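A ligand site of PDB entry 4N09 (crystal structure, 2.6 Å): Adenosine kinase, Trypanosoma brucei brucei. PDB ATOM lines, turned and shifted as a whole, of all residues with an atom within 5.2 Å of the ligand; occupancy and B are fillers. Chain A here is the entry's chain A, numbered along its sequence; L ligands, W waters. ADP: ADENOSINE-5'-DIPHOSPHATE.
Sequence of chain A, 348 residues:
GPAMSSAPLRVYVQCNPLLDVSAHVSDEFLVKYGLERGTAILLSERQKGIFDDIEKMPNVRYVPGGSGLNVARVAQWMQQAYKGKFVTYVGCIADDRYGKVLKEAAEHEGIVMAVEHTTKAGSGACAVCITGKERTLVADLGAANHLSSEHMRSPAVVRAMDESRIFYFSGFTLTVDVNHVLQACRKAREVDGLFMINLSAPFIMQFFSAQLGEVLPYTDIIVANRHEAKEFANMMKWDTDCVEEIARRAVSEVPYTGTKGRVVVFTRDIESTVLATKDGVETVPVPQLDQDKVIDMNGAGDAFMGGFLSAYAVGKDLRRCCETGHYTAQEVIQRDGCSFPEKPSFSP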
ATOM      1  N   ASN A 225     -11.993 -17.045  -1.925  1.00  0.00           N
ATOM      2  CA  ASN A 225     -12.319 -17.014  -3.360  1.00  0.00           C
ATOM      3  C   ASN A 225     -11.125 -16.595  -4.228  1.00  0.00           C
ATOM      4  O   ASN A 225     -10.033 -16.326  -3.727  1.00  0.00           O
ATOM      5  CB  ASN A 225     -13.530 -16.101  -3.616  1.00  0.00           C
ATOM      6  CG  ASN A 225     -13.209 -14.644  -3.353  1.00  0.00           C
ATOM      7  OD1 ASN A 225     -12.077 -14.190  -3.506  1.00  0.00           O
ATOM      8  ND2 ASN A 225     -14.206 -13.905  -2.984  1.00  0.00           N
ATOM      9  N   GLU A 228      -9.456 -13.038  -3.512  1.00  0.00           N
ATOM     10  CA  GLU A 228      -8.763 -13.072  -2.237  1.00  0.00           C
ATOM     11  C   GLU A 228      -7.475 -13.872  -2.334  1.00  0.00           C
ATOM     12  O   GLU A 228      -6.480 -13.564  -1.682  1.00  0.00           O
ATOM     13  CB  GLU A 228      -9.680 -13.667  -1.159  1.00  0.00           C
ATOM     14  CG  GLU A 228     -10.861 -12.767  -0.817  1.00  0.00           C
ATOM     15  CD  GLU A 228     -12.118 -13.486  -0.280  1.00  0.00           C
ATOM     16  OE1 GLU A 228     -12.091 -14.719  -0.053  1.00  0.00           O
ATOM     17  OE2 GLU A 228     -13.147 -12.786  -0.116  1.00  0.00           O
ATOM     18  N   THR A 267     -12.546 -21.070  -3.875  1.00  0.00           N
ATOM     19  CA  THR A 267     -13.655 -21.128  -4.795  1.00  0.00           C
ATOM     20  C   THR A 267     -13.386 -20.204  -5.989  1.00  0.00           C
ATOM     21  O   THR A 267     -12.505 -19.345  -5.928  1.00  0.00           O
ATOM     22  CB  THR A 267     -14.987 -20.741  -4.150  1.00  0.00           C
ATOM     23  OG1 THR A 267     -14.876 -19.432  -3.562  1.00  0.00           O
ATOM     24  CG2 THR A 267     -15.346 -21.743  -3.088  1.00  0.00           C
ATOM     25  N   ARG A 268     -14.148 -20.392  -7.071  1.00  0.00           N
ATOM     26  CA  ARG A 268     -13.922 -19.671  -8.325  1.00  0.00           C
ATOM     27  C   ARG A 268     -15.207 -19.509  -9.085  1.00  0.00           C
ATOM     28  O   ARG A 268     -15.283 -19.796 -10.272  1.00  0.00           O
ATOM     29  CB  ARG A 268     -12.947 -20.452  -9.196  1.00  0.00           C
ATOM     30  CG  ARG A 268     -11.558 -20.583  -8.568  1.00  0.00           C
ATOM     31  CD  ARG A 268     -10.514 -20.947  -9.598  1.00  0.00           C
ATOM     32  NE  ARG A 268     -10.650 -22.321 -10.040  1.00  0.00           N
ATOM     33  CZ  ARG A 268      -9.807 -22.925 -10.855  1.00  0.00           C
ATOM     34  NH1 ARG A 268      -8.766 -22.270 -11.338  1.00  0.00           N
ATOM     35  NH2 ARG A 268      -9.992 -24.204 -11.172  1.00  0.00           N
ATOM     36  N   ASP A 269     -16.249 -19.062  -8.391  1.00  0.00           N
ATOM     37  CA  ASP A 269     -17.579 -18.896  -8.974  1.00  0.00           C
ATOM     38  C   ASP A 269     -17.960 -20.043  -9.938  1.00  0.00           C
ATOM     39  O   ASP A 269     -18.125 -21.158  -9.480  1.00  0.00           O
ATOM     40  CB  ASP A 269     -17.792 -17.474  -9.566  1.00  0.00           C
ATOM     41  CG  ASP A 269     -16.710 -17.034 -10.546  1.00  0.00           C
ATOM     42  OD1 ASP A 269     -15.689 -16.425 -10.102  1.00  0.00           O
ATOM     43  OD2 ASP A 269     -16.899 -17.288 -11.770  1.00  0.00           O
ATOM     44  N   ILE A 270     -18.065 -19.759 -11.237  1.00  0.00           N
ATOM     45  CA  ILE A 270     -18.553 -20.730 -12.226  1.00  0.00           C
ATOM     46  C   ILE A 270     -17.562 -21.880 -12.379  1.00  0.00           C
ATOM     47  O   ILE A 270     -17.964 -22.977 -12.746  1.00  0.00           O
ATOM     48  CB  ILE A 270     -18.829 -20.040 -13.615  1.00  0.00           C
ATOM     49  CG1 ILE A 270     -20.211 -19.359 -13.647  1.00  0.00           C
ATOM     50  CG2 ILE A 270     -18.742 -21.004 -14.788  1.00  0.00           C
ATOM     51  CD1 ILE A 270     -20.587 -18.730 -14.994  1.00  0.00           C
ATOM     52  N   GLU A 271     -16.272 -21.617 -12.155  1.00  0.00           N
ATOM     53  CA  GLU A 271     -15.233 -22.614 -12.364  1.00  0.00           C
ATOM     54  C   GLU A 271     -14.977 -23.467 -11.157  1.00  0.00           C
ATOM     55  O   GLU A 271     -15.376 -23.148 -10.029  1.00  0.00           O
ATOM     56  CB  GLU A 271     -13.922 -21.916 -12.731  1.00  0.00           C
ATOM     57  CG  GLU A 271     -13.781 -21.582 -14.205  1.00  0.00           C
ATOM     58  CD  GLU A 271     -13.036 -20.285 -14.407  1.00  0.00           C
ATOM     59  OE1 GLU A 271     -11.825 -20.270 -14.761  1.00  0.00           O
ATOM     60  OE2 GLU A 271     -13.659 -19.265 -14.141  1.00  0.00           O
ATOM     61  N   THR A 273     -13.668 -25.553  -7.956  1.00  0.00           N
ATOM     62  CA  THR A 273     -13.076 -25.186  -6.706  1.00  0.00           C
ATOM     63  C   THR A 273     -11.742 -25.911  -6.548  1.00  0.00           C
ATOM     64  O   THR A 273     -11.631 -27.106  -6.801  1.00  0.00           O
ATOM     65  CB  THR A 273     -14.039 -25.544  -5.560  1.00  0.00           C
ATOM     66  OG1 THR A 273     -15.175 -24.667  -5.619  1.00  0.00           O
ATOM     67  CG2 THR A 273     -13.365 -25.388  -4.211  1.00  0.00           C
ATOM     68  N   VAL A 286     -18.000 -27.416 -10.341  1.00  0.00           N
ATOM     69  CA  VAL A 286     -19.230 -26.775  -9.934  1.00  0.00           C
ATOM     70  C   VAL A 286     -20.315 -27.207 -10.896  1.00  0.00           C
ATOM     71  O   VAL A 286     -20.212 -26.928 -12.072  1.00  0.00           O
ATOM     72  CB  VAL A 286     -19.089 -25.242 -10.020  1.00  0.00           C
ATOM     73  CG1 VAL A 286     -20.421 -24.554  -9.767  1.00  0.00           C
ATOM     74  CG2 VAL A 286     -18.053 -24.748  -9.034  1.00  0.00           C
ATOM     75  N   PRO A 287     -21.390 -27.808 -10.402  1.00  0.00           N
ATOM     76  CA  PRO A 287     -22.468 -28.234 -11.306  1.00  0.00           C
ATOM     77  C   PRO A 287     -22.971 -27.087 -12.180  1.00  0.00           C
ATOM     78  O   PRO A 287     -23.180 -25.983 -11.674  1.00  0.00           O
ATOM     79  CB  PRO A 287     -23.566 -28.663 -10.337  1.00  0.00           C
ATOM     80  CG  PRO A 287     -22.891 -28.975  -9.069  1.00  0.00           C
ATOM     81  CD  PRO A 287     -21.719 -28.054  -8.984  1.00  0.00           C
ATOM     82  N   LEU A 289     -25.308 -24.520 -14.047  1.00  0.00           N
ATOM     83  CA  LEU A 289     -26.554 -23.893 -13.629  1.00  0.00           C
ATOM     84  C   LEU A 289     -26.909 -22.806 -14.649  1.00  0.00           C
ATOM     85  O   LEU A 289     -26.063 -21.996 -14.988  1.00  0.00           O
ATOM     86  CB  LEU A 289     -26.363 -23.306 -12.207  1.00  0.00           C
ATOM     87  CG  LEU A 289     -27.511 -22.485 -11.656  1.00  0.00           C
ATOM     88  CD1 LEU A 289     -28.738 -23.328 -11.379  1.00  0.00           C
ATOM     89  CD2 LEU A 289     -27.075 -21.753 -10.414  1.00  0.00           C
ATOM     90  N   GLN A 291     -27.643 -19.539 -16.032  1.00  0.00           N
ATOM     91  CA  GLN A 291     -27.279 -18.276 -15.380  1.00  0.00           C
ATOM     92  C   GLN A 291     -28.434 -17.321 -15.212  1.00  0.00           C
ATOM     93  O   GLN A 291     -28.372 -16.389 -14.429  1.00  0.00           O
ATOM     94  CB  GLN A 291     -26.117 -17.610 -16.108  1.00  0.00           C
ATOM     95  CG  GLN A 291     -24.819 -18.409 -16.004  1.00  0.00           C
ATOM     96  CD  GLN A 291     -24.411 -18.687 -14.547  1.00  0.00           C
ATOM     97  OE1 GLN A 291     -23.952 -17.795 -13.850  1.00  0.00           O
ATOM     98  NE2 GLN A 291     -24.585 -19.918 -14.090  1.00  0.00           N
ATOM     99  N   VAL A 294     -29.667 -17.406 -11.752  1.00  0.00           N
ATOM    100  CA  VAL A 294     -28.809 -16.762 -10.787  1.00  0.00           C
ATOM    101  C   VAL A 294     -29.187 -15.278 -10.649  1.00  0.00           C
ATOM    102  O   VAL A 294     -28.923 -14.487 -11.533  1.00  0.00           O
ATOM    103  CB  VAL A 294     -27.345 -16.858 -11.210  1.00  0.00           C
ATOM    104  CG1 VAL A 294     -26.471 -16.109 -10.213  1.00  0.00           C
ATOM    105  CG2 VAL A 294     -26.898 -18.308 -11.299  1.00  0.00           C
ATOM    106  N   MET A 297     -25.599 -12.841  -6.364  1.00  0.00           N
ATOM    107  CA  MET A 297     -24.242 -13.346  -6.172  1.00  0.00           C
ATOM    108  C   MET A 297     -23.787 -13.196  -4.725  1.00  0.00           C
ATOM    109  O   MET A 297     -22.800 -13.781  -4.305  1.00  0.00           O
ATOM    110  CB  MET A 297     -23.256 -12.554  -7.026  1.00  0.00           C
ATOM    111  CG  MET A 297     -23.396 -12.746  -8.523  1.00  0.00           C
ATOM    112  SD  MET A 297     -23.344 -14.509  -8.911  1.00  0.00           S
ATOM    113  CE  MET A 297     -21.657 -14.950  -8.436  1.00  0.00           C
ATOM    114  N   GLY A 299     -23.183 -13.273  -0.859  1.00  0.00           N
ATOM    115  CA  GLY A 299     -23.230 -14.311   0.138  1.00  0.00           C
ATOM    116  C   GLY A 299     -23.013 -15.716  -0.390  1.00  0.00           C
ATOM    117  O   GLY A 299     -23.122 -16.658   0.366  1.00  0.00           O
ATOM    118  N   ALA A 300     -22.695 -15.876  -1.677  1.00  0.00           N
ATOM    119  CA  ALA A 300     -22.440 -17.213  -2.205  1.00  0.00           C
ATOM    120  C   ALA A 300     -21.354 -17.910  -1.407  1.00  0.00           C
ATOM    121  O   ALA A 300     -21.481 -19.104  -1.098  1.00  0.00           O
ATOM    122  CB  ALA A 300     -22.044 -17.154  -3.657  1.00  0.00           C
ATOM    123  N   GLY A 301     -20.295 -17.161  -1.100  1.00  0.00           N
ATOM    124  CA  GLY A 301     -19.172 -17.671  -0.330  1.00  0.00           C
ATOM    125  C   GLY A 301     -19.593 -18.075   1.070  1.00  0.00           C
ATOM    126  O   GLY A 301     -19.183 -19.125   1.552  1.00  0.00           O
ATOM    127  N   ASP A 302     -20.427 -17.253   1.704  1.00  0.00           N
ATOM    128  CA  ASP A 302     -20.940 -17.574   3.031  1.00  0.00           C
ATOM    129  C   ASP A 302     -21.757 -18.873   2.949  1.00  0.00           C
ATOM    130  O   ASP A 302     -21.681 -19.721   3.823  1.00  0.00           O
ATOM    131  CB  ASP A 302     -21.831 -16.470   3.569  1.00  0.00           C
ATOM    132  CG  ASP A 302     -21.098 -15.152   3.817  1.00  0.00           C
ATOM    133  OD1 ASP A 302     -19.869 -15.151   3.988  1.00  0.00           O
ATOM    134  OD2 ASP A 302     -21.777 -14.092   3.870  1.00  0.00           O
ATOM    135  N   PHE A 304     -21.465 -21.237   0.732  1.00  0.00           N
ATOM    136  CA  PHE A 304     -20.548 -22.336   0.457  1.00  0.00           C
ATOM    137  C   PHE A 304     -19.933 -22.840   1.757  1.00  0.00           C
ATOM    138  O   PHE A 304     -19.891 -24.028   2.030  1.00  0.00           O
ATOM    139  CB  PHE A 304     -19.449 -21.885  -0.509  1.00  0.00           C
ATOM    140  CG  PHE A 304     -18.371 -22.890  -0.687  1.00  0.00           C
ATOM    141  CD1 PHE A 304     -18.535 -23.896  -1.597  1.00  0.00           C
ATOM    142  CD2 PHE A 304     -17.252 -22.876   0.105  1.00  0.00           C
ATOM    143  CE1 PHE A 304     -17.573 -24.872  -1.730  1.00  0.00           C
ATOM    144  CE2 PHE A 304     -16.269 -23.845  -0.023  1.00  0.00           C
ATOM    145  CZ  PHE A 304     -16.426 -24.835  -0.948  1.00  0.00           C
ATOM    146  N   GLY A 325     -20.960 -27.663  -0.123  1.00  0.00           N
ATOM    147  CA  GLY A 325     -20.852 -26.205  -0.295  1.00  0.00           C
ATOM    148  C   GLY A 325     -21.370 -25.717  -1.642  1.00  0.00           C
ATOM    149  O   GLY A 325     -22.056 -24.716  -1.707  1.00  0.00           O
ATOM    150  N   HIS A 326     -21.063 -26.408  -2.722  1.00  0.00           N
ATOM    151  CA  HIS A 326     -21.605 -26.034  -4.007  1.00  0.00           C
ATOM    152  C   HIS A 326     -23.103 -26.104  -3.980  1.00  0.00           C
ATOM    153  O   HIS A 326     -23.775 -25.247  -4.571  1.00  0.00           O
ATOM    154  CB  HIS A 326     -21.065 -26.945  -5.108  1.00  0.00           C
ATOM    155  CG  HIS A 326     -19.594 -26.769  -5.353  1.00  0.00           C
ATOM    156  ND1 HIS A 326     -18.837 -27.681  -6.050  1.00  0.00           N
ATOM    157  CD2 HIS A 326     -18.737 -25.788  -4.970  1.00  0.00           C
ATOM    158  CE1 HIS A 326     -17.591 -27.258  -6.120  1.00  0.00           C
ATOM    159  NE2 HIS A 326     -17.495 -26.124  -5.454  1.00  0.00           N
ATOM    160  N   ALA A 329     -24.494 -23.088  -1.921  1.00  0.00           N
ATOM    161  CA  ALA A 329     -24.235 -21.804  -2.585  1.00  0.00           C
ATOM    162  C   ALA A 329     -25.150 -21.645  -3.760  1.00  0.00           C
ATOM    163  O   ALA A 329     -25.673 -20.559  -3.980  1.00  0.00           O
ATOM    164  CB  ALA A 329     -22.811 -21.707  -3.037  1.00  0.00           C
ATOM    165  N   GLN A 330     -25.389 -22.739  -4.467  1.00  0.00           N
ATOM    166  CA  GLN A 330     -26.279 -22.696  -5.618  1.00  0.00           C
ATOM    167  C   GLN A 330     -27.765 -22.554  -5.234  1.00  0.00           C
ATOM    168  O   GLN A 330     -28.550 -22.030  -5.998  1.00  0.00           O
ATOM    169  CB  GLN A 330     -26.024 -23.894  -6.541  1.00  0.00           C
ATOM    170  CG  GLN A 330     -24.705 -23.746  -7.267  1.00  0.00           C
ATOM    171  CD  GLN A 330     -24.527 -24.716  -8.399  1.00  0.00           C
ATOM    172  OE1 GLN A 330     -25.198 -25.741  -8.466  1.00  0.00           O
ATOM    173  NE2 GLN A 330     -23.617 -24.413  -9.288  1.00  0.00           N
ATOM    174  N   ILE A 333     -28.012 -18.457  -4.387  1.00  0.00           N
ATOM    175  CA  ILE A 333     -27.881 -17.506  -5.463  1.00  0.00           C
ATOM    176  C   ILE A 333     -29.149 -17.481  -6.333  1.00  0.00           C
ATOM    177  O   ILE A 333     -29.339 -16.543  -7.106  1.00  0.00           O
ATOM    178  CB  ILE A 333     -26.594 -17.709  -6.297  1.00  0.00           C
ATOM    179  CG1 ILE A 333     -26.574 -19.059  -6.988  1.00  0.00           C
ATOM    180  CG2 ILE A 333     -25.386 -17.517  -5.428  1.00  0.00           C
ATOM    181  CD1 ILE A 333     -25.309 -19.319  -7.783  1.00  0.00           C
HETATM  182  PB  ADP L   1     -17.859 -15.406  -3.257  1.00  0.00           P
HETATM  183  O1B ADP L   1     -16.829 -15.375  -2.114  1.00  0.00           O
HETATM  184  O2B ADP L   1     -19.316 -15.177  -2.851  1.00  0.00           O
HETATM  185  O3B ADP L   1     -17.514 -14.586  -4.491  1.00  0.00           O
HETATM  186  PA  ADP L   1     -17.689 -17.491  -5.200  1.00  0.00           P
HETATM  187  O1A ADP L   1     -18.292 -16.381  -6.054  1.00  0.00           O
HETATM  188  O2A ADP L   1     -16.343 -18.128  -5.550  1.00  0.00           O
HETATM  189  O3A ADP L   1     -17.687 -16.960  -3.682  1.00  0.00           O
HETATM  190  O5' ADP L   1     -18.796 -18.682  -5.180  1.00  0.00           O
HETATM  191  C5' ADP L   1     -18.926 -19.608  -4.126  1.00  0.00           C
HETATM  192  C4' ADP L   1     -19.614 -20.768  -4.747  1.00  0.00           C
HETATM  193  O4' ADP L   1     -20.907 -20.361  -5.126  1.00  0.00           O
HETATM  194  C3' ADP L   1     -18.918 -21.282  -6.007  1.00  0.00           C
HETATM  195  O3' ADP L   1     -17.864 -22.205  -5.719  1.00  0.00           O
HETATM  196  C2' ADP L   1     -20.092 -21.884  -6.726  1.00  0.00           C
HETATM  197  O2' ADP L   1     -20.370 -23.140  -6.186  1.00  0.00           O
HETATM  198  C1' ADP L   1     -21.268 -21.007  -6.349  1.00  0.00           C
HETATM  199  N9  ADP L   1     -21.495 -19.978  -7.396  1.00  0.00           N
HETATM  200  C8  ADP L   1     -21.094 -18.696  -7.317  1.00  0.00           C
HETATM  201  N7  ADP L   1     -21.465 -18.031  -8.422  1.00  0.00           N
HETATM  202  C5  ADP L   1     -22.104 -18.875  -9.224  1.00  0.00           C
HETATM  203  C6  ADP L   1     -22.750 -18.791 -10.547  1.00  0.00           C
HETATM  204  N6  ADP L   1     -22.765 -17.618 -11.208  1.00  0.00           N
HETATM  205  N1  ADP L   1     -23.304 -19.916 -11.069  1.00  0.00           N
HETATM  206  C2  ADP L   1     -23.291 -21.077 -10.402  1.00  0.00           C
HETATM  207  N3  ADP L   1     -22.726 -21.181  -9.197  1.00  0.00           N
HETATM  208  C4  ADP L   1     -22.127 -20.150  -8.571  1.00  0.00           C
HETATM  209  O   HOH W   1     -15.911 -22.520  -7.137  1.00  0.00           O
HETATM  210  O   HOH W   2     -15.563 -13.605   0.322  1.00  0.00           O
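O2B of the ligand sits at hydrogen-bond distance from N of Gly 301 (2.8 Å). OE1 of Gln 291 is in hydrogen-bond range of N6 of the ligand, at 2.9 Å. O2A of the ligand sits at hydrogen-bond distance from N of Asp 269 (3.0 Å). A nitrogen (N3) of the ligand is in hydrogen-bond range of the side-chain amide nitrogen (NE2) of Gln 330, at 3.4 Å. The side-chain amide nitrogen (ND2) of Asn 225 is in hydrogen-bond range of an oxygen (O1B) of the ligand (3.1 Å). OG1 of Thr 267 sits at hydrogen-bond distance from O2A of the ligand (2.8 Å).
The side-chain amide nitrogen (NE2) of Gln 330 sits at hydrogen-bond distance from the backbone carbonyl oxygen (O) of Pro 287. The side-chain amide oxygen (OD1) of Asn 225 sits at hydrogen-bond distance from the backbone NH (N) of Glu 228 (2.9 Å). A ring nitrogen (NE2) of His 326 sits at hydrogen-bond distance from the side-chain hydroxyl of Thr 273, 2.7 Å away. The backbone carbonyl oxygen (O) of Leu 289 sits at hydrogen-bond distance from the side-chain amide nitrogen (NE2) of Gln 291 (2.7 Å).
Merely in contact with the ligand: Met 297 (3.1 Å), Ala 329 (3.1 Å), His 326 (3.3 Å), Ile 333 (3.4 Å), Ala 300 (3.5 Å), Arg 268 (3.5 Å), Thr 273 (3.6 Å), Leu 289 (3.8 Å), Val 286 (3.9 Å), Ile 270 (3.9 Å) and Val 294 (3.9 Å). Hydrophobic or aromatic side chains within 4 Å of the ligand: Ile 270, Val 286, Leu 289, Val 294, Met 297, Ala 300, His 326, Ala 329 and Ile 333. Within 4 Å of the ligand: Asn 225, Thr 267, Arg 268, Asp 269, Ile 270, Thr 273, Val 286, Leu 289, Gln 291, Val 294, Met 297, Ala 300, Gly 301, His 326, Ala 329, Gln 330 and Ile 333. The nearest printed residue that does not touch the ligand is Phe 304 (4.3 Å).
Water W1 lies within hydrogen-bond range of O3' of the ligand (2.4 Å), OG1 of Thr 273 (2.7 Å), N of Arg 268 (2.8 Å) and O of Glu 271 (3.0 Å). Water W2 bridges the side-chain carboxylate (OE2) of Glu 228 (2.6 Å) and an oxygen (O1B) of the ligand (3.3 Å).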
